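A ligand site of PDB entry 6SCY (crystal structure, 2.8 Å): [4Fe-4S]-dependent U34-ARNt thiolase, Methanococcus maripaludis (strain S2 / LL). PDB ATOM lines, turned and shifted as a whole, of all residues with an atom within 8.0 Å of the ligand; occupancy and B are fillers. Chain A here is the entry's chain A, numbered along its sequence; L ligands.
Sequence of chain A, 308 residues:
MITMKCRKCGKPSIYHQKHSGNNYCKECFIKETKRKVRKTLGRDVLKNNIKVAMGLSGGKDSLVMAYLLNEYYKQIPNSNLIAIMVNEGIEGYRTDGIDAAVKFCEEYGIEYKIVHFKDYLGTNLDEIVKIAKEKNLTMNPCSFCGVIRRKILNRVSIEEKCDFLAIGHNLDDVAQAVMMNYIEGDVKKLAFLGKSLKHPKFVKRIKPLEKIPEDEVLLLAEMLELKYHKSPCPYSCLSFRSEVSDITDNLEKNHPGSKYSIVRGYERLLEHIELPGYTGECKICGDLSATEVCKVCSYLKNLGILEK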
ATOM      1  N   VAL A  86     -22.499  11.175  10.402  1.00  0.00           N
ATOM      2  CA  VAL A  86     -21.381  10.919  11.311  1.00  0.00           C
ATOM      3  C   VAL A  86     -21.568  11.632  12.651  1.00  0.00           C
ATOM      4  O   VAL A  86     -21.387  12.846  12.722  1.00  0.00           O
ATOM      5  CB  VAL A  86     -19.993  11.217  10.658  1.00  0.00           C
ATOM      6  CG1 VAL A  86     -18.857  10.682  11.521  1.00  0.00           C
ATOM      7  CG2 VAL A  86     -19.889  10.651   9.250  1.00  0.00           C
ATOM      8  N   GLU A  88     -20.216  12.877  15.729  1.00  0.00           N
ATOM      9  CA  GLU A  88     -18.895  13.192  16.265  1.00  0.00           C
ATOM     10  C   GLU A  88     -18.746  12.798  17.744  1.00  0.00           C
ATOM     11  O   GLU A  88     -17.629  12.711  18.240  1.00  0.00           O
ATOM     12  CB  GLU A  88     -18.533  14.673  16.031  1.00  0.00           C
ATOM     13  CG  GLU A  88     -18.335  15.017  14.562  1.00  0.00           C
ATOM     14  CD  GLU A  88     -19.376  15.909  13.920  1.00  0.00           C
ATOM     15  OE1 GLU A  88     -20.476  16.084  14.490  1.00  0.00           O
ATOM     16  OE2 GLU A  88     -19.089  16.442  12.824  1.00  0.00           O
ATOM     17  N   ILE A  90     -19.305  14.482  20.261  1.00  0.00           N
ATOM     18  CA  ILE A  90     -18.935  15.659  21.055  1.00  0.00           C
ATOM     19  C   ILE A  90     -20.192  16.233  21.734  1.00  0.00           C
ATOM     20  O   ILE A  90     -20.634  17.333  21.414  1.00  0.00           O
ATOM     21  CB  ILE A  90     -18.110  16.712  20.237  1.00  0.00           C
ATOM     22  CG1 ILE A  90     -17.096  16.055  19.244  1.00  0.00           C
ATOM     23  CG2 ILE A  90     -17.370  17.696  21.163  1.00  0.00           C
ATOM     24  CD1 ILE A  90     -16.478  17.007  18.177  1.00  0.00           C
ATOM     25  N   ARG A  94     -26.248  17.144  18.844  1.00  0.00           N
ATOM     26  CA  ARG A  94     -25.898  16.769  17.465  1.00  0.00           C
ATOM     27  C   ARG A  94     -26.985  15.820  16.992  1.00  0.00           C
ATOM     28  O   ARG A  94     -27.308  15.792  15.803  1.00  0.00           O
ATOM     29  CB  ARG A  94     -24.552  16.023  17.429  1.00  0.00           C
ATOM     30  CG  ARG A  94     -23.372  16.838  17.988  1.00  0.00           C
ATOM     31  CD  ARG A  94     -22.066  16.295  17.472  1.00  0.00           C
ATOM     32  NE  ARG A  94     -20.986  17.258  17.690  1.00  0.00           N
ATOM     33  CZ  ARG A  94     -20.675  18.243  16.858  1.00  0.00           C
ATOM     34  NH1 ARG A  94     -21.361  18.426  15.740  1.00  0.00           N
ATOM     35  NH2 ARG A  94     -19.672  19.057  17.137  1.00  0.00           N
ATOM     36  N   PHE A 117     -17.862   8.421  15.574  1.00  0.00           N
ATOM     37  CA  PHE A 117     -16.440   8.761  15.651  1.00  0.00           C
ATOM     38  C   PHE A 117     -15.767   7.750  16.593  1.00  0.00           C
ATOM     39  O   PHE A 117     -14.660   7.284  16.324  1.00  0.00           O
ATOM     40  CB  PHE A 117     -16.279  10.203  16.207  1.00  0.00           C
ATOM     41  CG  PHE A 117     -15.866  11.289  15.241  1.00  0.00           C
ATOM     42  CD1 PHE A 117     -16.562  11.490  14.053  1.00  0.00           C
ATOM     43  CD2 PHE A 117     -14.832  12.166  15.551  1.00  0.00           C
ATOM     44  CE1 PHE A 117     -16.192  12.519  13.171  1.00  0.00           C
ATOM     45  CE2 PHE A 117     -14.483  13.199  14.678  1.00  0.00           C
ATOM     46  CZ  PHE A 117     -15.160  13.361  13.496  1.00  0.00           C
ATOM     47  N   ASN A 124     -13.829  10.681  21.391  1.00  0.00           N
ATOM     48  CA  ASN A 124     -14.247  12.042  21.035  1.00  0.00           C
ATOM     49  C   ASN A 124     -15.559  12.490  21.722  1.00  0.00           C
ATOM     50  O   ASN A 124     -16.288  13.321  21.190  1.00  0.00           O
ATOM     51  CB  ASN A 124     -14.286  12.311  19.521  1.00  0.00           C
ATOM     52  CG  ASN A 124     -14.137  13.790  19.173  1.00  0.00           C
ATOM     53  OD1 ASN A 124     -13.764  14.633  19.999  1.00  0.00           O
ATOM     54  ND2 ASN A 124     -14.467  14.149  17.950  1.00  0.00           N
ATOM     55  N   ILE A 128     -10.990  16.970  23.008  1.00  0.00           N
ATOM     56  CA  ILE A 128     -10.044  18.077  23.195  1.00  0.00           C
ATOM     57  C   ILE A 128     -10.061  18.504  24.686  1.00  0.00           C
ATOM     58  O   ILE A 128     -10.819  19.378  25.095  1.00  0.00           O
ATOM     59  CB  ILE A 128     -10.260  19.239  22.165  1.00  0.00           C
ATOM     60  CG1 ILE A 128     -10.342  18.716  20.688  1.00  0.00           C
ATOM     61  CG2 ILE A 128      -9.208  20.363  22.311  1.00  0.00           C
ATOM     62  CD1 ILE A 128      -9.058  18.008  20.051  1.00  0.00           C
ATOM     63  N   LEU A 137     -12.854  26.955   9.062  1.00  0.00           N
ATOM     64  CA  LEU A 137     -11.987  25.896   9.585  1.00  0.00           C
ATOM     65  C   LEU A 137     -10.509  26.264   9.435  1.00  0.00           C
ATOM     66  O   LEU A 137     -10.071  26.589   8.326  1.00  0.00           O
ATOM     67  CB  LEU A 137     -12.281  24.557   8.887  1.00  0.00           C
ATOM     68  CG  LEU A 137     -13.602  23.866   9.252  1.00  0.00           C
ATOM     69  CD1 LEU A 137     -14.637  24.085   8.177  1.00  0.00           C
ATOM     70  CD2 LEU A 137     -13.401  22.393   9.475  1.00  0.00           C
ATOM     71  N   ASN A 140      -6.480  22.968  15.325  1.00  0.00           N
ATOM     72  CA  ASN A 140      -6.635  22.258  16.602  1.00  0.00           C
ATOM     73  C   ASN A 140      -8.040  21.607  16.857  1.00  0.00           C
ATOM     74  O   ASN A 140      -8.121  20.425  16.491  1.00  0.00           O
ATOM     75  CB  ASN A 140      -6.183  23.070  17.811  1.00  0.00           C
ATOM     76  CG  ASN A 140      -5.959  22.216  19.043  1.00  0.00           C
ATOM     77  OD1 ASN A 140      -5.151  21.275  19.038  1.00  0.00           O
ATOM     78  ND2 ASN A 140      -6.665  22.516  20.130  1.00  0.00           N
ATOM     79  N   PRO A 141      -9.091  22.146  17.545  1.00  0.00           N
ATOM     80  CA  PRO A 141     -10.290  21.325  17.760  1.00  0.00           C
ATOM     81  C   PRO A 141     -11.197  21.158  16.543  1.00  0.00           C
ATOM     82  O   PRO A 141     -11.550  20.025  16.207  1.00  0.00           O
ATOM     83  CB  PRO A 141     -11.000  21.996  18.947  1.00  0.00           C
ATOM     84  CG  PRO A 141     -10.197  23.226  19.285  1.00  0.00           C
ATOM     85  CD  PRO A 141      -9.294  23.495  18.127  1.00  0.00           C
ATOM     86  N   CYS A 142     -11.572  22.275  15.902  1.00  0.00           N
ATOM     87  CA  CYS A 142     -12.447  22.288  14.728  1.00  0.00           C
ATOM     88  C   CYS A 142     -11.814  21.621  13.515  1.00  0.00           C
ATOM     89  O   CYS A 142     -12.515  20.946  12.772  1.00  0.00           O
ATOM     90  CB  CYS A 142     -12.911  23.705  14.407  1.00  0.00           C
ATOM     91  SG  CYS A 142     -14.337  23.802  13.298  1.00  0.00           S
ATOM     92  N   SER A 143     -10.488  21.800  13.336  1.00  0.00           N
ATOM     93  CA  SER A 143      -9.721  21.208  12.231  1.00  0.00           C
ATOM     94  C   SER A 143      -9.639  19.684  12.358  1.00  0.00           C
ATOM     95  O   SER A 143      -9.952  18.989  11.391  1.00  0.00           O
ATOM     96  CB  SER A 143      -8.326  21.803  12.137  1.00  0.00           C
ATOM     97  OG  SER A 143      -7.453  21.299  13.138  1.00  0.00           O
ATOM     98  N   PHE A 144      -9.239  19.167  13.548  1.00  0.00           N
ATOM     99  CA  PHE A 144      -9.109  17.737  13.829  1.00  0.00           C
ATOM    100  C   PHE A 144     -10.416  16.991  13.576  1.00  0.00           C
ATOM    101  O   PHE A 144     -10.383  15.874  13.052  1.00  0.00           O
ATOM    102  CB  PHE A 144      -8.590  17.487  15.251  1.00  0.00           C
ATOM    103  CG  PHE A 144      -8.541  16.034  15.685  1.00  0.00           C
ATOM    104  CD1 PHE A 144      -7.615  15.156  15.145  1.00  0.00           C
ATOM    105  CD2 PHE A 144      -9.411  15.560  16.658  1.00  0.00           C
ATOM    106  CE1 PHE A 144      -7.568  13.824  15.545  1.00  0.00           C
ATOM    107  CE2 PHE A 144      -9.368  14.216  17.064  1.00  0.00           C
ATOM    108  CZ  PHE A 144      -8.448  13.365  16.507  1.00  0.00           C
ATOM    109  N   CYS A 145     -11.553  17.615  13.929  1.00  0.00           N
ATOM    110  CA  CYS A 145     -12.879  17.061  13.717  1.00  0.00           C
ATOM    111  C   CYS A 145     -13.223  16.910  12.228  1.00  0.00           C
ATOM    112  O   CYS A 145     -13.714  15.860  11.822  1.00  0.00           O
ATOM    113  CB  CYS A 145     -13.941  17.874  14.445  1.00  0.00           C
ATOM    114  SG  CYS A 145     -15.632  17.298  14.183  1.00  0.00           S
ATOM    115  N   GLY A 146     -12.963  17.952  11.444  1.00  0.00           N
ATOM    116  CA  GLY A 146     -13.207  17.964  10.005  1.00  0.00           C
ATOM    117  C   GLY A 146     -12.333  16.992   9.227  1.00  0.00           C
ATOM    118  O   GLY A 146     -12.803  16.378   8.267  1.00  0.00           O
ATOM    119  N   VAL A 147     -11.054  16.840   9.651  1.00  0.00           N
ATOM    120  CA  VAL A 147     -10.061  15.940   9.044  1.00  0.00           C
ATOM    121  C   VAL A 147     -10.471  14.482   9.233  1.00  0.00           C
ATOM    122  O   VAL A 147     -10.491  13.725   8.258  1.00  0.00           O
ATOM    123  CB  VAL A 147      -8.605  16.259   9.534  1.00  0.00           C
ATOM    124  CG1 VAL A 147      -7.615  15.160   9.118  1.00  0.00           C
ATOM    125  CG2 VAL A 147      -8.128  17.612   9.021  1.00  0.00           C
ATOM    126  N   ARG A 149     -13.617  13.304  10.116  1.00  0.00           N
ATOM    127  CA  ARG A 149     -14.906  13.174   9.421  1.00  0.00           C
ATOM    128  C   ARG A 149     -14.703  12.746   7.953  1.00  0.00           C
ATOM    129  O   ARG A 149     -15.396  11.854   7.470  1.00  0.00           O
ATOM    130  CB  ARG A 149     -15.704  14.491   9.501  1.00  0.00           C
ATOM    131  CG  ARG A 149     -17.084  14.461   8.856  1.00  0.00           C
ATOM    132  CD  ARG A 149     -18.026  15.519   9.416  1.00  0.00           C
ATOM    133  NE  ARG A 149     -17.735  16.863   8.909  1.00  0.00           N
ATOM    134  CZ  ARG A 149     -17.178  17.831   9.620  1.00  0.00           C
ATOM    135  NH1 ARG A 149     -16.847  17.621  10.900  1.00  0.00           N
ATOM    136  NH2 ARG A 149     -16.955  19.016   9.081  1.00  0.00           N
ATOM    137  N   SER A 231     -28.444  22.534  13.705  1.00  0.00           N
ATOM    138  CA  SER A 231     -27.213  21.804  14.047  1.00  0.00           C
ATOM    139  C   SER A 231     -26.018  22.724  14.474  1.00  0.00           C
ATOM    140  O   SER A 231     -25.014  22.812  13.755  1.00  0.00           O
ATOM    141  CB  SER A 231     -26.815  20.810  12.945  1.00  0.00           C
ATOM    142  OG  SER A 231     -26.980  21.293  11.623  1.00  0.00           O
ATOM    143  N   PRO A 232     -26.098  23.385  15.657  1.00  0.00           N
ATOM    144  CA  PRO A 232     -24.983  24.235  16.098  1.00  0.00           C
ATOM    145  C   PRO A 232     -23.916  23.476  16.900  1.00  0.00           C
ATOM    146  O   PRO A 232     -24.242  22.498  17.572  1.00  0.00           O
ATOM    147  CB  PRO A 232     -25.668  25.313  16.941  1.00  0.00           C
ATOM    148  CG  PRO A 232     -26.954  24.684  17.420  1.00  0.00           C
ATOM    149  CD  PRO A 232     -27.205  23.414  16.645  1.00  0.00           C
ATOM    150  N   CYS A 233     -22.653  23.922  16.820  1.00  0.00           N
ATOM    151  CA  CYS A 233     -21.553  23.252  17.512  1.00  0.00           C
ATOM    152  C   CYS A 233     -21.258  23.823  18.914  1.00  0.00           C
ATOM    153  O   CYS A 233     -20.907  25.002  19.026  1.00  0.00           O
ATOM    154  CB  CYS A 233     -20.297  23.219  16.639  1.00  0.00           C
ATOM    155  SG  CYS A 233     -18.998  22.122  17.265  1.00  0.00           S
ATOM    156  N   PRO A 234     -21.383  22.994  19.989  1.00  0.00           N
ATOM    157  CA  PRO A 234     -21.102  23.504  21.344  1.00  0.00           C
ATOM    158  C   PRO A 234     -19.629  23.512  21.744  1.00  0.00           C
ATOM    159  O   PRO A 234     -19.307  24.021  22.823  1.00  0.00           O
ATOM    160  CB  PRO A 234     -21.946  22.593  22.256  1.00  0.00           C
ATOM    161  CG  PRO A 234     -22.363  21.421  21.417  1.00  0.00           C
ATOM    162  CD  PRO A 234     -21.792  21.581  20.036  1.00  0.00           C
ATOM    163  N   TYR A 235     -18.731  22.967  20.889  1.00  0.00           N
ATOM    164  CA  TYR A 235     -17.296  22.897  21.190  1.00  0.00           C
ATOM    165  C   TYR A 235     -16.388  23.532  20.113  1.00  0.00           C
ATOM    166  O   TYR A 235     -15.158  23.416  20.222  1.00  0.00           O
ATOM    167  CB  TYR A 235     -16.870  21.453  21.492  1.00  0.00           C
ATOM    168  CG  TYR A 235     -17.014  21.067  22.957  1.00  0.00           C
ATOM    169  CD1 TYR A 235     -15.944  21.195  23.841  1.00  0.00           C
ATOM    170  CD2 TYR A 235     -18.227  20.608  23.463  1.00  0.00           C
ATOM    171  CE1 TYR A 235     -16.069  20.874  25.184  1.00  0.00           C
ATOM    172  CE2 TYR A 235     -18.363  20.281  24.817  1.00  0.00           C
ATOM    173  CZ  TYR A 235     -17.287  20.413  25.666  1.00  0.00           C
ATOM    174  OH  TYR A 235     -17.413  20.080  27.001  1.00  0.00           O
ATOM    175  N   SER A 236     -16.971  24.234  19.111  1.00  0.00           N
ATOM    176  CA  SER A 236     -16.198  24.917  18.064  1.00  0.00           C
ATOM    177  C   SER A 236     -16.890  26.123  17.430  1.00  0.00           C
ATOM    178  O   SER A 236     -18.026  26.041  16.954  1.00  0.00           O
ATOM    179  CB  SER A 236     -15.734  23.951  16.976  1.00  0.00           C
ATOM    180  OG  SER A 236     -14.589  23.218  17.387  1.00  0.00           O
ATOM    181  N   CYS A 237     -16.163  27.266  17.455  1.00  0.00           N
ATOM    182  CA  CYS A 237     -16.543  28.568  16.919  1.00  0.00           C
ATOM    183  C   CYS A 237     -15.285  29.349  16.493  1.00  0.00           C
ATOM    184  O   CYS A 237     -14.645  30.017  17.321  1.00  0.00           O
ATOM    185  CB  CYS A 237     -17.401  29.361  17.907  1.00  0.00           C
ATOM    186  SG  CYS A 237     -17.770  31.059  17.386  1.00  0.00           S
ATOM    187  N   LEU A 238     -14.928  29.240  15.207  1.00  0.00           N
ATOM    188  CA  LEU A 238     -13.792  29.942  14.596  1.00  0.00           C
ATOM    189  C   LEU A 238     -14.315  31.223  13.999  1.00  0.00           C
ATOM    190  O   LEU A 238     -15.137  31.185  13.081  1.00  0.00           O
ATOM    191  CB  LEU A 238     -13.114  29.083  13.529  1.00  0.00           C
ATOM    192  CG  LEU A 238     -11.629  29.414  13.330  1.00  0.00           C
ATOM    193  CD1 LEU A 238     -10.846  28.104  13.417  1.00  0.00           C
ATOM    194  CD2 LEU A 238     -11.381  30.122  11.979  1.00  0.00           C
HETATM  195 FE1  LIG L   1     -15.640  22.009  14.070  1.00  0.00          FE
HETATM  196 FE2  LIG L   1     -16.323  19.339  14.166  1.00  0.00          FE
HETATM  197 FE3  LIG L   1     -17.886  21.096  12.754  1.00  0.00          FE
HETATM  198 FE4  LIG L   1     -17.852  21.207  15.496  1.00  0.00          FE
HETATM  199  S1  LIG L   1     -18.613  19.470  14.190  1.00  0.00           S
HETATM  200  S2  LIG L   1     -17.717  22.986  14.058  1.00  0.00           S
HETATM  201  S3  LIG L   1     -15.657  20.663  15.929  1.00  0.00           S
HETATM  202  S4  LIG L   1     -15.707  20.527  12.304  1.00  0.00           S
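SG of Cys 145 binds FE2 of the ligand, 2.2 Å away.
FE4 of the ligand is bound by SG of Cys 233, at 2.3 Å.
An iron atom (FE1) of the ligand is bound by the side-chain sulfur (SG) of Cys 142 (2.3 Å).
OG of Ser 236 lies close to S3 of the ligand (3.1 Å).
The guanidinium group of Arg 94 lies close to a sulfur (S1) of the ligand (3.2 Å).
A sulfur (S4) of the ligand sits close to the guanidinium group (NH1) of Arg 149.
OE2 of Glu 88 lies close to S1 of the ligand, at 3.4 Å.
Gly 146 touches the ligand (N to S4, 3.9 Å).
Within 4 Å of the ligand: Glu 88, Arg 94, Cys 142, Cys 145, Gly 146, Arg 149, Cys 233 and Ser 236.
Along chain A the residues within 4 Å of the ligand span positions 88 to 236.
The nearest printed residue that does not touch the ligand is Leu 137 (4.1 Å).
NH1 of Arg 149 lies close to SG of Cys 145 (3.5 Å).
The side-chain sulfur (SG) of Cys 233 sits close to the backbone NH (N) of Ser 236 (3.5 Å).
SG of Cys 233 lies close to NH2 of Arg 94, 3.1 Å away.
The side-chain sulfur (SG) of Cys 233 sits close to the backbone NH (N) of Tyr 235, 3.7 Å away.
The backbone NH of Cys 142 lies close to the side-chain hydroxyl of Ser 236, at 3.5 Å.
NH1 of Arg 94 lies within salt-bridge range of OE1 of Glu 88 (2.8 Å).
OE2 of Glu 88 is in salt-bridge range of NH1 of Arg 149, at 3.2 Å.
ND2 of Asn 124 sits at hydrogen-bond distance from O of Glu 88, at 3.5 Å.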
